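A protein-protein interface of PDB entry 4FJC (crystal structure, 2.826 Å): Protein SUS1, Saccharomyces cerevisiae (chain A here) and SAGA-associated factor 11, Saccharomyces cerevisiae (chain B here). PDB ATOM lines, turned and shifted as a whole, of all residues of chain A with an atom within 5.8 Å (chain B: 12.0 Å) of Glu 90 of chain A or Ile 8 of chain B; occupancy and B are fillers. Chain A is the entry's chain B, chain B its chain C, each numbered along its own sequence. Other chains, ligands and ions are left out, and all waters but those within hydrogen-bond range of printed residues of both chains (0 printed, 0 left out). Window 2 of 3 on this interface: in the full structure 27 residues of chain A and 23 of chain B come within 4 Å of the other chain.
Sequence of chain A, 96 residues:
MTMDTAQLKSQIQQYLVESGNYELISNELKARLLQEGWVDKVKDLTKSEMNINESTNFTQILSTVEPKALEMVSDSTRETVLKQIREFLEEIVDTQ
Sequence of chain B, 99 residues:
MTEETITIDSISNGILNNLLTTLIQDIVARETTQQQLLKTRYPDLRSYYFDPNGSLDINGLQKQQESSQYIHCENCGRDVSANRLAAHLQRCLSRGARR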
ATOM      1  N   ILE A  85      15.223 -20.772 -17.226  1.00  0.00           N
ATOM      2  CA  ILE A  85      15.750 -21.384 -15.996  1.00  0.00           C
ATOM      3  C   ILE A  85      17.036 -22.187 -16.243  1.00  0.00           C
ATOM      4  O   ILE A  85      17.993 -22.094 -15.466  1.00  0.00           O
ATOM      5  CB  ILE A  85      14.705 -22.270 -15.286  1.00  0.00           C
ATOM      6  CG1 ILE A  85      13.492 -21.447 -14.859  1.00  0.00           C
ATOM      7  CG2 ILE A  85      15.269 -22.859 -14.011  1.00  0.00           C
ATOM      8  CD1 ILE A  85      12.342 -22.264 -14.303  1.00  0.00           C
ATOM      9  N   ARG A  86      17.052 -22.965 -17.320  1.00  0.00           N
ATOM     10  CA  ARG A  86      18.264 -23.669 -17.766  1.00  0.00           C
ATOM     11  C   ARG A  86      19.412 -22.723 -18.089  1.00  0.00           C
ATOM     12  O   ARG A  86      20.529 -22.938 -17.630  1.00  0.00           O
ATOM     13  CB  ARG A  86      17.989 -24.507 -19.014  1.00  0.00           C
ATOM     14  CG  ARG A  86      17.043 -25.658 -18.791  1.00  0.00           C
ATOM     15  CD  ARG A  86      17.320 -26.792 -19.766  1.00  0.00           C
ATOM     16  NE  ARG A  86      17.457 -26.342 -21.157  1.00  0.00           N
ATOM     17  CZ  ARG A  86      16.444 -26.119 -21.995  1.00  0.00           C
ATOM     18  NH1 ARG A  86      15.172 -26.298 -21.616  1.00  0.00           N
ATOM     19  NH2 ARG A  86      16.716 -25.704 -23.227  1.00  0.00           N
ATOM     20  N   GLU A  87      19.148 -21.699 -18.898  1.00  0.00           N
ATOM     21  CA  GLU A  87      20.170 -20.694 -19.203  1.00  0.00           C
ATOM     22  C   GLU A  87      20.773 -20.130 -17.927  1.00  0.00           C
ATOM     23  O   GLU A  87      21.959 -19.848 -17.866  1.00  0.00           O
ATOM     24  CB  GLU A  87      19.602 -19.532 -20.013  1.00  0.00           C
ATOM     25  CG  GLU A  87      19.299 -19.812 -21.478  1.00  0.00           C
ATOM     26  CD  GLU A  87      18.488 -18.682 -22.103  1.00  0.00           C
ATOM     27  OE1 GLU A  87      17.348 -18.417 -21.633  1.00  0.00           O
ATOM     28  OE2 GLU A  87      18.987 -18.041 -23.050  1.00  0.00           O
ATOM     29  N   PHE A  88      19.953 -19.951 -16.899  1.00  0.00           N
ATOM     30  CA  PHE A  88      20.480 -19.498 -15.609  1.00  0.00           C
ATOM     31  C   PHE A  88      21.257 -20.601 -14.861  1.00  0.00           C
ATOM     32  O   PHE A  88      22.293 -20.339 -14.272  1.00  0.00           O
ATOM     33  CB  PHE A  88      19.352 -18.972 -14.736  1.00  0.00           C
ATOM     34  CG  PHE A  88      18.813 -17.640 -15.154  1.00  0.00           C
ATOM     35  CD1 PHE A  88      19.638 -16.533 -15.217  1.00  0.00           C
ATOM     36  CD2 PHE A  88      17.455 -17.473 -15.402  1.00  0.00           C
ATOM     37  CE1 PHE A  88      19.130 -15.293 -15.576  1.00  0.00           C
ATOM     38  CE2 PHE A  88      16.937 -16.236 -15.754  1.00  0.00           C
ATOM     39  CZ  PHE A  88      17.773 -15.142 -15.849  1.00  0.00           C
ATOM     40  N   LEU A  89      20.768 -21.829 -14.882  1.00  0.00           N
ATOM     41  CA  LEU A  89      21.446 -22.897 -14.152  1.00  0.00           C
ATOM     42  C   LEU A  89      22.858 -23.172 -14.672  1.00  0.00           C
ATOM     43  O   LEU A  89      23.738 -23.550 -13.892  1.00  0.00           O
ATOM     44  CB  LEU A  89      20.628 -24.196 -14.160  1.00  0.00           C
ATOM     45  CG  LEU A  89      19.385 -24.263 -13.269  1.00  0.00           C
ATOM     46  CD1 LEU A  89      19.001 -25.713 -13.098  1.00  0.00           C
ATOM     47  CD2 LEU A  89      19.637 -23.633 -11.918  1.00  0.00           C
ATOM     48  N   GLU A  90      23.069 -22.973 -15.974  1.00  0.00           N
ATOM     49  CA  GLU A  90      24.367 -23.222 -16.616  1.00  0.00           C
ATOM     50  C   GLU A  90      25.486 -22.253 -16.246  1.00  0.00           C
ATOM     51  O   GLU A  90      26.651 -22.636 -16.201  1.00  0.00           O
ATOM     52  CB  GLU A  90      24.197 -23.215 -18.122  1.00  0.00           C
ATOM     53  CG  GLU A  90      23.502 -24.460 -18.621  1.00  0.00           C
ATOM     54  CD  GLU A  90      23.073 -24.316 -20.054  1.00  0.00           C
ATOM     55  OE1 GLU A  90      23.676 -23.481 -20.777  1.00  0.00           O
ATOM     56  OE2 GLU A  90      22.124 -25.034 -20.445  1.00  0.00           O
ATOM     57  N   GLU A  91      25.154 -20.998 -15.992  1.00  0.00           N
ATOM     58  CA  GLU A  91      26.154 -20.078 -15.473  1.00  0.00           C
ATOM     59  C   GLU A  91      26.735 -20.547 -14.122  1.00  0.00           C
ATOM     60  O   GLU A  91      27.836 -20.122 -13.764  1.00  0.00           O
ATOM     61  CB  GLU A  91      25.580 -18.662 -15.346  1.00  0.00           C
ATOM     62  CG  GLU A  91      25.343 -17.967 -16.690  1.00  0.00           C
ATOM     63  CD  GLU A  91      24.434 -16.741 -16.582  1.00  0.00           C
ATOM     64  OE1 GLU A  91      23.361 -16.844 -15.942  1.00  0.00           O
ATOM     65  OE2 GLU A  91      24.788 -15.679 -17.152  1.00  0.00           O
ATOM     66  N   ILE A  92      26.033 -21.426 -13.388  1.00  0.00           N
ATOM     67  CA  ILE A  92      26.484 -21.810 -12.038  1.00  0.00           C
ATOM     68  C   ILE A  92      26.697 -23.291 -11.736  1.00  0.00           C
ATOM     69  O   ILE A  92      27.258 -23.632 -10.701  1.00  0.00           O
ATOM     70  CB  ILE A  92      25.532 -21.243 -10.972  1.00  0.00           C
ATOM     71  CG1 ILE A  92      24.179 -21.945 -11.012  1.00  0.00           C
ATOM     72  CG2 ILE A  92      25.348 -19.746 -11.184  1.00  0.00           C
ATOM     73  CD1 ILE A  92      23.308 -21.588  -9.843  1.00  0.00           C
ATOM     74  N   VAL A  93      26.239 -24.174 -12.606  1.00  0.00           N
ATOM     75  CA  VAL A  93      26.283 -25.618 -12.331  1.00  0.00           C
ATOM     76  C   VAL A  93      27.181 -26.358 -13.315  1.00  0.00           C
ATOM     77  O   VAL A  93      27.012 -26.221 -14.537  1.00  0.00           O
ATOM     78  CB  VAL A  93      24.863 -26.223 -12.360  1.00  0.00           C
ATOM     79  CG1 VAL A  93      24.860 -27.618 -12.956  1.00  0.00           C
ATOM     80  CG2 VAL A  93      24.282 -26.236 -10.956  1.00  0.00           C
ATOM     81  N   THR A  95      28.723 -29.918 -14.985  1.00  0.00           N
ATOM     82  CA  THR A  95      27.911 -30.985 -15.571  1.00  0.00           C
ATOM     83  C   THR A  95      28.518 -32.370 -15.260  1.00  0.00           C
ATOM     84  O   THR A  95      29.512 -32.444 -14.535  1.00  0.00           O
ATOM     85  CB  THR A  95      27.778 -30.700 -17.102  1.00  0.00           C
ATOM     86  OG1 THR A  95      26.420 -30.888 -17.534  1.00  0.00           O
ATOM     87  CG2 THR A  95      28.788 -31.512 -17.955  1.00  0.00           C
ATOM     88  N   GLU B   4      18.611 -41.538  -7.936  1.00  0.00           N
ATOM     89  CA  GLU B   4      18.298 -41.256  -9.343  1.00  0.00           C
ATOM     90  C   GLU B   4      18.939 -39.976  -9.866  1.00  0.00           C
ATOM     91  O   GLU B   4      19.399 -39.126  -9.098  1.00  0.00           O
ATOM     92  CB  GLU B   4      16.777 -41.192  -9.562  1.00  0.00           C
ATOM     93  CG  GLU B   4      16.045 -42.520  -9.369  1.00  0.00           C
ATOM     94  CD  GLU B   4      16.362 -43.566 -10.433  1.00  0.00           C
ATOM     95  OE1 GLU B   4      17.508 -43.629 -10.928  1.00  0.00           O
ATOM     96  OE2 GLU B   4      15.450 -44.348 -10.766  1.00  0.00           O
ATOM     97  N   THR B   5      18.940 -39.857 -11.193  1.00  0.00           N
ATOM     98  CA  THR B   5      19.678 -38.816 -11.909  1.00  0.00           C
ATOM     99  C   THR B   5      19.072 -37.420 -11.742  1.00  0.00           C
ATOM    100  O   THR B   5      17.914 -37.193 -12.124  1.00  0.00           O
ATOM    101  CB  THR B   5      19.748 -39.156 -13.419  1.00  0.00           C
ATOM    102  OG1 THR B   5      20.571 -40.317 -13.610  1.00  0.00           O
ATOM    103  CG2 THR B   5      20.313 -37.992 -14.232  1.00  0.00           C
ATOM    104  N   ILE B   6      19.861 -36.495 -11.184  1.00  0.00           N
ATOM    105  CA  ILE B   6      19.486 -35.079 -11.157  1.00  0.00           C
ATOM    106  C   ILE B   6      20.153 -34.337 -12.332  1.00  0.00           C
ATOM    107  O   ILE B   6      21.353 -34.118 -12.362  1.00  0.00           O
ATOM    108  CB  ILE B   6      19.717 -34.420  -9.765  1.00  0.00           C
ATOM    109  CG1 ILE B   6      21.122 -33.840  -9.597  1.00  0.00           C
ATOM    110  CG2 ILE B   6      19.420 -35.418  -8.653  1.00  0.00           C
ATOM    111  CD1 ILE B   6      21.387 -33.329  -8.201  1.00  0.00           C
ATOM    112  N   THR B   7      19.347 -33.984 -13.321  1.00  0.00           N
ATOM    113  CA  THR B   7      19.840 -33.347 -14.534  1.00  0.00           C
ATOM    114  C   THR B   7      19.560 -31.837 -14.525  1.00  0.00           C
ATOM    115  O   THR B   7      18.904 -31.304 -13.627  1.00  0.00           O
ATOM    116  CB  THR B   7      19.237 -34.010 -15.814  1.00  0.00           C
ATOM    117  OG1 THR B   7      19.120 -33.049 -16.878  1.00  0.00           O
ATOM    118  CG2 THR B   7      17.861 -34.597 -15.559  1.00  0.00           C
ATOM    119  N   ILE B   8      20.086 -31.156 -15.536  1.00  0.00           N
ATOM    120  CA  ILE B   8      19.719 -29.774 -15.801  1.00  0.00           C
ATOM    121  C   ILE B   8      18.221 -29.667 -16.068  1.00  0.00           C
ATOM    122  O   ILE B   8      17.577 -28.737 -15.585  1.00  0.00           O
ATOM    123  CB  ILE B   8      20.491 -29.205 -17.008  1.00  0.00           C
ATOM    124  CG1 ILE B   8      21.906 -28.796 -16.585  1.00  0.00           C
ATOM    125  CG2 ILE B   8      19.746 -28.018 -17.608  1.00  0.00           C
ATOM    126  CD1 ILE B   8      22.630 -27.940 -17.612  1.00  0.00           C
ATOM    127  N   ASP B   9      17.681 -30.613 -16.839  1.00  0.00           N
ATOM    128  CA  ASP B   9      16.238 -30.671 -17.119  1.00  0.00           C
ATOM    129  C   ASP B   9      15.416 -30.900 -15.854  1.00  0.00           C
ATOM    130  O   ASP B   9      14.363 -30.284 -15.689  1.00  0.00           O
ATOM    131  CB  ASP B   9      15.900 -31.789 -18.125  1.00  0.00           C
ATOM    132  CG  ASP B   9      16.240 -31.422 -19.580  1.00  0.00           C
ATOM    133  OD1 ASP B   9      16.543 -30.231 -19.870  1.00  0.00           O
ATOM    134  OD2 ASP B   9      16.189 -32.343 -20.442  1.00  0.00           O
ATOM    135  N   SER B  10      15.888 -31.785 -14.968  1.00  0.00           N
ATOM    136  CA  SER B  10      15.086 -32.181 -13.808  1.00  0.00           C
ATOM    137  C   SER B  10      15.044 -31.084 -12.751  1.00  0.00           C
ATOM    138  O   SER B  10      13.973 -30.797 -12.238  1.00  0.00           O
ATOM    139  CB  SER B  10      15.561 -33.501 -13.194  1.00  0.00           C
ATOM    140  OG  SER B  10      16.699 -33.307 -12.384  1.00  0.00           O
ATOM    141  N   ILE B  11      16.184 -30.477 -12.420  1.00  0.00           N
ATOM    142  CA  ILE B  11      16.182 -29.387 -11.454  1.00  0.00           C
ATOM    143  C   ILE B  11      15.375 -28.227 -11.999  1.00  0.00           C
ATOM    144  O   ILE B  11      14.643 -27.572 -11.256  1.00  0.00           O
ATOM    145  CB  ILE B  11      17.600 -28.875 -11.098  1.00  0.00           C
ATOM    146  CG1 ILE B  11      18.296 -29.822 -10.112  1.00  0.00           C
ATOM    147  CG2 ILE B  11      17.539 -27.489 -10.462  1.00  0.00           C
ATOM    148  CD1 ILE B  11      17.592 -29.972  -8.775  1.00  0.00           C
ATOM    149  N   SER B  12      15.513 -27.975 -13.298  1.00  0.00           N
ATOM    150  CA  SER B  12      14.779 -26.889 -13.947  1.00  0.00           C
ATOM    151  C   SER B  12      13.271 -27.070 -13.812  1.00  0.00           C
ATOM    152  O   SER B  12      12.552 -26.106 -13.542  1.00  0.00           O
ATOM    153  CB  SER B  12      15.136 -26.795 -15.429  1.00  0.00           C
ATOM    154  OG  SER B  12      16.394 -26.204 -15.613  1.00  0.00           O
ATOM    155  N   ASN B  13      12.807 -28.302 -14.033  1.00  0.00           N
ATOM    156  CA  ASN B  13      11.398 -28.647 -13.936  1.00  0.00           C
ATOM    157  C   ASN B  13      10.977 -28.571 -12.472  1.00  0.00           C
ATOM    158  O   ASN B  13       9.836 -28.271 -12.163  1.00  0.00           O
ATOM    159  CB  ASN B  13      11.136 -30.049 -14.517  1.00  0.00           C
ATOM    160  CG  ASN B  13      11.047 -30.070 -16.054  1.00  0.00           C
ATOM    161  OD1 ASN B  13      10.314 -29.299 -16.668  1.00  0.00           O
ATOM    162  ND2 ASN B  13      11.759 -30.998 -16.669  1.00  0.00           N
ATOM    163  N   GLY B  14      11.911 -28.801 -11.563  1.00  0.00           N
ATOM    164  CA  GLY B  14      11.642 -28.623 -10.143  1.00  0.00           C
ATOM    165  C   GLY B  14      11.371 -27.181  -9.780  1.00  0.00           C
ATOM    166  O   GLY B  14      10.484 -26.873  -9.010  1.00  0.00           O
ATOM    167  N   ILE B  15      12.145 -26.284 -10.348  1.00  0.00           N
ATOM    168  CA  ILE B  15      11.963 -24.885 -10.073  1.00  0.00           C
ATOM    169  C   ILE B  15      10.652 -24.370 -10.691  1.00  0.00           C
ATOM    170  O   ILE B  15       9.936 -23.547 -10.079  1.00  0.00           O
ATOM    171  CB  ILE B  15      13.161 -24.104 -10.590  1.00  0.00           C
ATOM    172  CG1 ILE B  15      14.403 -24.539  -9.826  1.00  0.00           C
ATOM    173  CG2 ILE B  15      12.937 -22.633 -10.380  1.00  0.00           C
ATOM    174  CD1 ILE B  15      15.694 -24.118 -10.469  1.00  0.00           C
ATOM    175  N   LEU B  16      10.329 -24.873 -11.885  1.00  0.00           N
ATOM    176  CA  LEU B  16       9.070 -24.500 -12.554  1.00  0.00           C
ATOM    177  C   LEU B  16       7.829 -24.984 -11.814  1.00  0.00           C
ATOM    178  O   LEU B  16       6.817 -24.283 -11.788  1.00  0.00           O
ATOM    179  CB  LEU B  16       9.009 -25.008 -14.003  1.00  0.00           C
ATOM    180  CG  LEU B  16       7.703 -24.580 -14.709  1.00  0.00           C
ATOM    181  CD1 LEU B  16       7.502 -23.076 -14.643  1.00  0.00           C
ATOM    182  CD2 LEU B  16       7.642 -25.061 -16.146  1.00  0.00           C
ATOM    183  N   ASN B  17       7.907 -26.184 -11.235  1.00  0.00           N
ATOM    184  CA  ASN B  17       6.769 -26.798 -10.549  1.00  0.00           C
ATOM    185  C   ASN B  17       6.465 -26.114  -9.211  1.00  0.00           C
ATOM    186  O   ASN B  17       5.340 -25.792  -8.867  1.00  0.00           O
ATOM    187  CB  ASN B  17       7.088 -28.244 -10.321  1.00  0.00           C
ATOM    188  CG  ASN B  17       5.974 -28.970  -9.657  1.00  0.00           C
ATOM    189  OD1 ASN B  17       4.943 -29.206 -10.258  1.00  0.00           O
ATOM    190  ND2 ASN B  17       6.177 -29.345  -8.417  1.00  0.00           N
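The side-chain hydroxyl (OG) of Ser 12 of chain B lies within hydrogen-bond range of the backbone carbonyl oxygen (O) of Ile 8 of chain B, 2.8 Å away.
ND2 of Asn 13 of chain B lies within hydrogen-bond range of O of Asp 9 of chain B (2.9 Å).
The side-chain hydroxyl of Thr 7 of chain B lies within hydrogen-bond range of the backbone NH of Asp 9 of chain B.
OG of Ser 12 of chain B touches CG2 of Ile 85 of chain A, at 3.9 Å.
Ile 15 of chain B touches Ile 85 of chain A (CD1 to CG2, 3.8 Å).
Arg 86 of chain A touches Ile 8 of chain B.
CD of Arg 86 of chain A touches OD1 of Asp 9 of chain B, at 3.5 Å.
Arg 86 of chain A touches Ser 12 of chain B (CG to OG, 3.3 Å).
Ile 11 of chain B touches Leu 89 of chain A (CG2 to CD1, 3.5 Å).
OG of Ser 12 of chain B touches CD1 of Leu 89 of chain A, at 3.7 Å.
CG of Glu 90 of chain A touches CD1 of Ile 8 of chain B, 3.7 Å away.
Glu 90 of chain A touches just one residue of chain B: Ile 8 (3.7 Å).
Of chain A, only Arg 86 and Glu 90 come within 4 Å of Ile 8 of chain B.
Printed residues of chain B within 4 Å of Arg 86 of chain A: Ile 8 (3.5 Å), Asp 9 (3.5 Å) and Ser 12 (3.3 Å).
Of chain B, only Ile 11 and Ser 12 come within 4 Å of Leu 89 of chain A.
Glu 91 of chain A touches none of the printed residues of chain B.
Ile 92 of chain A touches none of the printed residues of chain B.
No residue of chain B comes within 4 Å of Val 93 of chain A.
Printed residues of chain A within 4 Å of Asp 9 of chain B: Arg 86.
Printed residues of chain B within 4 Å of Ile 85 of chain A: Ser 12 (3.9 Å) and Ile 15 (3.8 Å).
Printed residues of chain A within 4 Å of Ile 15 of chain B: Ile 85 (3.8 Å).
Printed residues of chain A within 4 Å of Ser 12 of chain B: Ile 85 (3.9 Å), Arg 86 (3.3 Å) and Leu 89 (3.7 Å).
Of the printed residues of chain A, Ile 11 of chain B touches Leu 89 (3.5 Å).
Asn 13 of chain B touches none of the printed residues of chain A.
Thr 95 of chain A touches none of the printed residues of chain B.
The nearest residue of chain B that does not touch Glu 90 of chain A is Ser 12 of chain B (7.4 Å).
The nearest printed residue of chain A that does not touch Asp 9 of chain B is Leu 89 of chain A (6.3 Å).
Hydrophobic or aromatic side chains of chain A within 4 Å of the printed part of chain B: Ile 85 and Leu 89.
Hydrophobic or aromatic side chains of chain B that line the printed part of chain A: Ile 8, Ile 11 and Ile 15.
Among the printed residues, 8 pairs touch across the chains.
Among the printed residues, no Asp or Glu carboxylate lies within 4 Å of a Lys or Arg side-chain nitrogen of the other chain.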
